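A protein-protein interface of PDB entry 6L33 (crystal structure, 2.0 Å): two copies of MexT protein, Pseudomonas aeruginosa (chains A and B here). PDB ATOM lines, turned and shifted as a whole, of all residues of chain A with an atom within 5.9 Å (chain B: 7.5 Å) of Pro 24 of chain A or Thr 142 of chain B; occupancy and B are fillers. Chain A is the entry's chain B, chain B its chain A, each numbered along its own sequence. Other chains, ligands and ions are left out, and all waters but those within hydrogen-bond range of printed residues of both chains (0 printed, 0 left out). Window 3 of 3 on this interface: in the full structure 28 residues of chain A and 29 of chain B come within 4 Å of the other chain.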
ATOM      1  N   GLU A  19     -29.431  -5.590  19.609  1.00  0.00           N
ATOM      2  CA  GLU A  19     -28.500  -6.712  19.654  1.00  0.00           C
ATOM      3  C   GLU A  19     -28.711  -7.592  20.884  1.00  0.00           C
ATOM      4  O   GLU A  19     -28.487  -8.806  20.821  1.00  0.00           O
ATOM      5  CB  GLU A  19     -27.066  -6.179  19.611  1.00  0.00           C
ATOM      6  CG  GLU A  19     -25.993  -7.224  19.800  1.00  0.00           C
ATOM      7  CD  GLU A  19     -24.691  -6.837  19.131  1.00  0.00           C
ATOM      8  OE1 GLU A  19     -23.662  -7.491  19.402  1.00  0.00           O
ATOM      9  OE2 GLU A  19     -24.701  -5.876  18.333  1.00  0.00           O
ATOM     10  N   PHE A  20     -29.155  -7.012  22.000  1.00  0.00           N
ATOM     11  CA  PHE A  20     -29.294  -7.788  23.229  1.00  0.00           C
ATOM     12  C   PHE A  20     -30.386  -8.846  23.104  1.00  0.00           C
ATOM     13  O   PHE A  20     -30.188 -10.004  23.487  1.00  0.00           O
ATOM     14  CB  PHE A  20     -29.580  -6.858  24.408  1.00  0.00           C
ATOM     15  CG  PHE A  20     -28.371  -6.120  24.898  1.00  0.00           C
ATOM     16  CD1 PHE A  20     -27.481  -6.723  25.774  1.00  0.00           C
ATOM     17  CD2 PHE A  20     -28.120  -4.826  24.480  1.00  0.00           C
ATOM     18  CE1 PHE A  20     -26.364  -6.043  26.225  1.00  0.00           C
ATOM     19  CE2 PHE A  20     -27.007  -4.142  24.924  1.00  0.00           C
ATOM     20  CZ  PHE A  20     -26.126  -4.751  25.799  1.00  0.00           C
ATOM     21  N   GLY A  21     -31.544  -8.467  22.571  1.00  0.00           N
ATOM     22  CA  GLY A  21     -32.661  -9.386  22.487  1.00  0.00           C
ATOM     23  C   GLY A  21     -32.686 -10.238  21.235  1.00  0.00           C
ATOM     24  O   GLY A  21     -33.053 -11.414  21.289  1.00  0.00           O
ATOM     25  N   LEU A  22     -32.288  -9.659  20.100  1.00  0.00           N
ATOM     26  CA  LEU A  22     -32.422 -10.347  18.820  1.00  0.00           C
ATOM     27  C   LEU A  22     -31.330 -11.390  18.614  1.00  0.00           C
ATOM     28  O   LEU A  22     -31.605 -12.489  18.118  1.00  0.00           O
ATOM     29  CB  LEU A  22     -32.399  -9.323  17.680  1.00  0.00           C
ATOM     30  CG  LEU A  22     -32.615  -9.776  16.231  1.00  0.00           C
ATOM     31  CD1 LEU A  22     -33.280  -8.661  15.442  1.00  0.00           C
ATOM     32  CD2 LEU A  22     -31.311 -10.181  15.558  1.00  0.00           C
ATOM     33  N   LEU A  23     -30.093 -11.061  18.983  1.00  0.00           N
ATOM     34  CA  LEU A  23     -28.951 -11.890  18.604  1.00  0.00           C
ATOM     35  C   LEU A  23     -28.977 -13.288  19.216  1.00  0.00           C
ATOM     36  O   LEU A  23     -28.770 -14.260  18.468  1.00  0.00           O
ATOM     37  CB  LEU A  23     -27.654 -11.144  18.945  1.00  0.00           C
ATOM     38  CG  LEU A  23     -26.425 -11.306  18.048  1.00  0.00           C
ATOM     39  CD1 LEU A  23     -25.319 -10.374  18.479  1.00  0.00           C
ATOM     40  CD2 LEU A  23     -25.924 -12.713  18.097  1.00  0.00           C
ATOM     41  N   PRO A  24     -29.192 -13.477  20.522  1.00  0.00           N
ATOM     42  CA  PRO A  24     -29.067 -14.830  21.103  1.00  0.00           C
ATOM     43  C   PRO A  24     -30.033 -15.828  20.478  1.00  0.00           C
ATOM     44  O   PRO A  24     -29.594 -16.908  20.052  1.00  0.00           O
ATOM     45  CB  PRO A  24     -29.353 -14.607  22.596  1.00  0.00           C
ATOM     46  CG  PRO A  24     -28.951 -13.199  22.831  1.00  0.00           C
ATOM     47  CD  PRO A  24     -29.341 -12.458  21.580  1.00  0.00           C
ATOM     48  N   PRO A  25     -31.341 -15.537  20.387  1.00  0.00           N
ATOM     49  CA  PRO A  25     -32.221 -16.514  19.729  1.00  0.00           C
ATOM     50  C   PRO A  25     -31.937 -16.662  18.247  1.00  0.00           C
ATOM     51  O   PRO A  25     -32.103 -17.759  17.701  1.00  0.00           O
ATOM     52  CB  PRO A  25     -33.626 -15.954  19.982  1.00  0.00           C
ATOM     53  CG  PRO A  25     -33.419 -14.504  20.112  1.00  0.00           C
ATOM     54  CD  PRO A  25     -32.116 -14.364  20.839  1.00  0.00           C
ATOM     55  N   LEU A  26     -31.505 -15.590  17.582  1.00  0.00           N
ATOM     56  CA  LEU A  26     -31.205 -15.675  16.159  1.00  0.00           C
ATOM     57  C   LEU A  26     -30.031 -16.610  15.902  1.00  0.00           C
ATOM     58  O   LEU A  26     -30.117 -17.519  15.070  1.00  0.00           O
ATOM     59  CB  LEU A  26     -30.919 -14.282  15.604  1.00  0.00           C
ATOM     60  CG  LEU A  26     -30.504 -14.239  14.136  1.00  0.00           C
ATOM     61  CD1 LEU A  26     -31.726 -14.265  13.222  1.00  0.00           C
ATOM     62  CD2 LEU A  26     -29.627 -13.033  13.858  1.00  0.00           C
ATOM     63  N   LEU A  27     -28.925 -16.406  16.627  1.00  0.00           N
ATOM     64  CA  LEU A  27     -27.729 -17.225  16.438  1.00  0.00           C
ATOM     65  C   LEU A  27     -28.037 -18.712  16.532  1.00  0.00           C
ATOM     66  O   LEU A  27     -27.486 -19.518  15.773  1.00  0.00           O
ATOM     67  CB  LEU A  27     -26.672 -16.851  17.474  1.00  0.00           C
ATOM     68  CG  LEU A  27     -25.532 -15.940  17.029  1.00  0.00           C
ATOM     69  CD1 LEU A  27     -24.427 -15.980  18.060  1.00  0.00           C
ATOM     70  CD2 LEU A  27     -25.004 -16.315  15.655  1.00  0.00           C
ATOM     71  N   ARG A  28     -28.913 -19.096  17.462  1.00  0.00           N
ATOM     72  CA  ARG A  28     -29.232 -20.507  17.639  1.00  0.00           C
ATOM     73  C   ARG A  28     -29.929 -21.088  16.415  1.00  0.00           C
ATOM     74  O   ARG A  28     -29.704 -22.256  16.074  1.00  0.00           O
ATOM     75  CB  ARG A  28     -30.096 -20.691  18.885  1.00  0.00           C
ATOM     76  CG  ARG A  28     -29.381 -20.355  20.183  1.00  0.00           C
ATOM     77  CD  ARG A  28     -30.254 -20.648  21.394  1.00  0.00           C
ATOM     78  NE  ARG A  28     -31.148 -19.537  21.710  1.00  0.00           N
ATOM     79  CZ  ARG A  28     -30.989 -18.723  22.748  1.00  0.00           C
ATOM     80  NH1 ARG A  28     -29.966 -18.892  23.574  1.00  0.00           N
ATOM     81  NH2 ARG A  28     -31.852 -17.738  22.961  1.00  0.00           N
ATOM     82  N   ARG A  29     -30.762 -20.296  15.734  1.00  0.00           N
ATOM     83  CA  ARG A  29     -31.484 -20.810  14.575  1.00  0.00           C
ATOM     84  C   ARG A  29     -30.542 -21.048  13.399  1.00  0.00           C
ATOM     85  O   ARG A  29     -30.551 -22.130  12.797  1.00  0.00           O
ATOM     86  CB  ARG A  29     -32.611 -19.851  14.184  1.00  0.00           C
ATOM     87  CG  ARG A  29     -33.609 -20.424  13.173  1.00  0.00           C
ATOM     88  CD  ARG A  29     -33.807 -21.925  13.368  1.00  0.00           C
ATOM     89  NE  ARG A  29     -35.180 -22.361  13.115  1.00  0.00           N
ATOM     90  CZ  ARG A  29     -35.657 -22.679  11.916  1.00  0.00           C
ATOM     91  NH1 ARG A  29     -34.876 -22.605  10.848  1.00  0.00           N
ATOM     92  NH2 ARG A  29     -36.916 -23.069  11.783  1.00  0.00           N
ATOM     93  N   ASN B 138     -20.866  -5.830  26.001  1.00  0.00           N
ATOM     94  CA  ASN B 138     -22.020  -5.924  26.883  1.00  0.00           C
ATOM     95  C   ASN B 138     -23.017  -6.941  26.341  1.00  0.00           C
ATOM     96  O   ASN B 138     -23.378  -6.910  25.161  1.00  0.00           O
ATOM     97  CB  ASN B 138     -22.682  -4.554  27.037  1.00  0.00           C
ATOM     98  CG  ASN B 138     -23.426  -4.406  28.354  1.00  0.00           C
ATOM     99  OD1 ASN B 138     -23.549  -5.361  29.124  1.00  0.00           O
ATOM    100  ND2 ASN B 138     -23.923  -3.204  28.619  1.00  0.00           N
ATOM    101  N   GLY B 139     -23.450  -7.850  27.208  1.00  0.00           N
ATOM    102  CA  GLY B 139     -24.342  -8.914  26.806  1.00  0.00           C
ATOM    103  C   GLY B 139     -23.664 -10.158  26.286  1.00  0.00           C
ATOM    104  O   GLY B 139     -24.354 -11.050  25.777  1.00  0.00           O
ATOM    105  N   LEU B 140     -22.333 -10.250  26.389  1.00  0.00           N
ATOM    106  CA  LEU B 140     -21.635 -11.455  25.952  1.00  0.00           C
ATOM    107  C   LEU B 140     -22.083 -12.677  26.740  1.00  0.00           C
ATOM    108  O   LEU B 140     -22.111 -13.788  26.198  1.00  0.00           O
ATOM    109  CB  LEU B 140     -20.123 -11.271  26.091  1.00  0.00           C
ATOM    110  CG  LEU B 140     -19.268 -11.139  24.830  1.00  0.00           C
ATOM    111  CD1 LEU B 140     -17.796 -11.280  25.184  1.00  0.00           C
ATOM    112  CD2 LEU B 140     -19.668 -12.157  23.772  1.00  0.00           C
ATOM    113  N   GLY B 141     -22.432 -12.494  28.017  1.00  0.00           N
ATOM    114  CA  GLY B 141     -22.871 -13.619  28.827  1.00  0.00           C
ATOM    115  C   GLY B 141     -24.116 -14.283  28.274  1.00  0.00           C
ATOM    116  O   GLY B 141     -24.146 -15.498  28.067  1.00  0.00           O
ATOM    117  N   THR B 142     -25.161 -13.492  28.023  1.00  0.00           N
ATOM    118  CA  THR B 142     -26.368 -14.037  27.411  1.00  0.00           C
ATOM    119  C   THR B 142     -26.104 -14.550  26.002  1.00  0.00           C
ATOM    120  O   THR B 142     -26.858 -15.396  25.507  1.00  0.00           O
ATOM    121  CB  THR B 142     -27.475 -12.979  27.387  1.00  0.00           C
ATOM    122  OG1 THR B 142     -27.442 -12.224  28.604  1.00  0.00           O
ATOM    123  CG2 THR B 142     -28.841 -13.635  27.248  1.00  0.00           C
ATOM    124  N   LEU B 143     -25.042 -14.072  25.353  1.00  0.00           N
ATOM    125  CA  LEU B 143     -24.722 -14.520  24.003  1.00  0.00           C
ATOM    126  C   LEU B 143     -24.089 -15.907  24.001  1.00  0.00           C
ATOM    127  O   LEU B 143     -24.409 -16.734  23.140  1.00  0.00           O
ATOM    128  CB  LEU B 143     -23.794 -13.512  23.325  1.00  0.00           C
ATOM    129  CG  LEU B 143     -23.476 -13.812  21.862  1.00  0.00           C
ATOM    130  CD1 LEU B 143     -24.762 -14.136  21.126  1.00  0.00           C
ATOM    131  CD2 LEU B 143     -22.752 -12.647  21.207  1.00  0.00           C
ATOM    132  N   LEU B 144     -23.188 -16.177  24.944  1.00  0.00           N
ATOM    133  CA  LEU B 144     -22.508 -17.463  25.028  1.00  0.00           C
ATOM    134  C   LEU B 144     -23.255 -18.478  25.885  1.00  0.00           C
ATOM    135  O   LEU B 144     -22.810 -19.627  25.981  1.00  0.00           O
ATOM    136  CB  LEU B 144     -21.090 -17.278  25.584  1.00  0.00           C
ATOM    137  CG  LEU B 144     -20.154 -16.289  24.885  1.00  0.00           C
ATOM    138  CD1 LEU B 144     -18.784 -16.290  25.551  1.00  0.00           C
ATOM    139  CD2 LEU B 144     -20.032 -16.611  23.406  1.00  0.00           C
ATOM    140  N   ALA B 145     -24.367 -18.085  26.503  1.00  0.00           N
ATOM    141  CA  ALA B 145     -25.067 -18.960  27.434  1.00  0.00           C
ATOM    142  C   ALA B 145     -25.531 -20.237  26.744  1.00  0.00           C
ATOM    143  O   ALA B 145     -26.113 -20.195  25.657  1.00  0.00           O
ATOM    144  CB  ALA B 145     -26.260 -18.227  28.048  1.00  0.00           C
ATOM    145  N   GLY B 146     -25.263 -21.374  27.383  1.00  0.00           N
ATOM    146  CA  GLY B 146     -25.664 -22.657  26.842  1.00  0.00           C
ATOM    147  C   GLY B 146     -24.896 -23.113  25.625  1.00  0.00           C
ATOM    148  O   GLY B 146     -25.325 -24.061  24.961  1.00  0.00           O
ATOM    149  N   THR B 147     -23.778 -22.468  25.306  1.00  0.00           N
ATOM    150  CA  THR B 147     -22.966 -22.815  24.150  1.00  0.00           C
ATOM    151  C   THR B 147     -21.553 -23.176  24.590  1.00  0.00           C
ATOM    152  O   THR B 147     -21.144 -22.930  25.729  1.00  0.00           O
ATOM    153  CB  THR B 147     -22.915 -21.662  23.136  1.00  0.00           C
ATOM    154  OG1 THR B 147     -21.970 -20.678  23.577  1.00  0.00           O
ATOM    155  CG2 THR B 147     -24.284 -21.010  22.984  1.00  0.00           C
ATOM    156  N   LEU B 161     -17.920  -8.439  33.006  1.00  0.00           N
ATOM    157  CA  LEU B 161     -18.800  -9.489  32.505  1.00  0.00           C
ATOM    158  C   LEU B 161     -18.995 -10.591  33.539  1.00  0.00           C
ATOM    159  O   LEU B 161     -20.110 -11.100  33.706  1.00  0.00           O
ATOM    160  CB  LEU B 161     -18.245 -10.057  31.199  1.00  0.00           C
ATOM    161  CG  LEU B 161     -18.619  -9.278  29.933  1.00  0.00           C
ATOM    162  CD1 LEU B 161     -17.635  -9.549  28.806  1.00  0.00           C
ATOM    163  CD2 LEU B 161     -20.039  -9.608  29.496  1.00  0.00           C
ATOM    164  N   GLY B 165     -22.520 -12.303  36.226  1.00  0.00           N
ATOM    165  CA  GLY B 165     -22.885 -13.691  36.416  1.00  0.00           C
ATOM    166  C   GLY B 165     -23.038 -14.447  35.106  1.00  0.00           C
ATOM    167  O   GLY B 165     -23.269 -13.878  34.041  1.00  0.00           O
ATOM    168  N   GLY B 166     -22.891 -15.770  35.202  1.00  0.00           N
ATOM    169  CA  GLY B 166     -23.131 -16.663  34.089  1.00  0.00           C
ATOM    170  C   GLY B 166     -21.901 -17.107  33.324  1.00  0.00           C
ATOM    171  O   GLY B 166     -22.028 -17.948  32.425  1.00  0.00           O
ATOM    172  N   LEU B 167     -20.721 -16.580  33.644  1.00  0.00           N
ATOM    173  CA  LEU B 167     -19.517 -16.884  32.884  1.00  0.00           C
ATOM    174  C   LEU B 167     -18.357 -17.196  33.819  1.00  0.00           C
ATOM    175  O   LEU B 167     -18.373 -16.857  35.004  1.00  0.00           O
ATOM    176  CB  LEU B 167     -19.123 -15.724  31.960  1.00  0.00           C
ATOM    177  CG  LEU B 167     -20.054 -15.357  30.806  1.00  0.00           C
ATOM    178  CD1 LEU B 167     -19.577 -14.064  30.164  1.00  0.00           C
ATOM    179  CD2 LEU B 167     -20.124 -16.478  29.780  1.00  0.00           C
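O of Pro 24 of chain A sits close to NE of Arg 28 of chain A, at 3.5 Å.
Phe 20 of chain A touches Asn 138 of chain B (CE1 to O, 3.3 Å).
Phe 20 of chain A touches Gly 139 of chain B (CE1 to CA, 3.6 Å).
Leu 23 of chain A touches Leu 143 of chain B.
CB of Pro 24 of chain A touches O of Thr 142 of chain B, at 3.9 Å.
CD1 of Leu 27 of chain A touches CD1 of Leu 143 of chain B (3.6 Å).
Pro 24 of chain A touches one residue of chain B.
Of the printed residues of chain A, Thr 142 of chain B touches Pro 24.
Printed residues of chain B within 4 Å of Leu 23 of chain A: Leu 143 (3.5 Å).
Of the printed residues of chain A, Leu 143 of chain B touches Leu 23 (3.5 Å) and Leu 27 (3.6 Å).
Of the printed residues of chain B, Phe 20 of chain A touches Asn 138 (3.3 Å) and Gly 139 (3.6 Å).
Of the printed residues of chain A, Gly 139 of chain B touches Phe 20.
Gly 146 of chain B touches none of the printed residues of chain A.
Hydrophobic or aromatic side chains of chain A that line the printed part of chain B: Phe 20, Leu 23, Pro 24 and Leu 27.
Hydrophobic or aromatic side chains of chain B within 4 Å of the printed part of chain A: Leu 143.
Among the printed residues, 5 pairs touch across the chains.
Among the printed residues, no Asp or Glu carboxylate lies within 4 Å of a Lys or Arg side-chain nitrogen of the other chain.
No position is printed for both chains.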
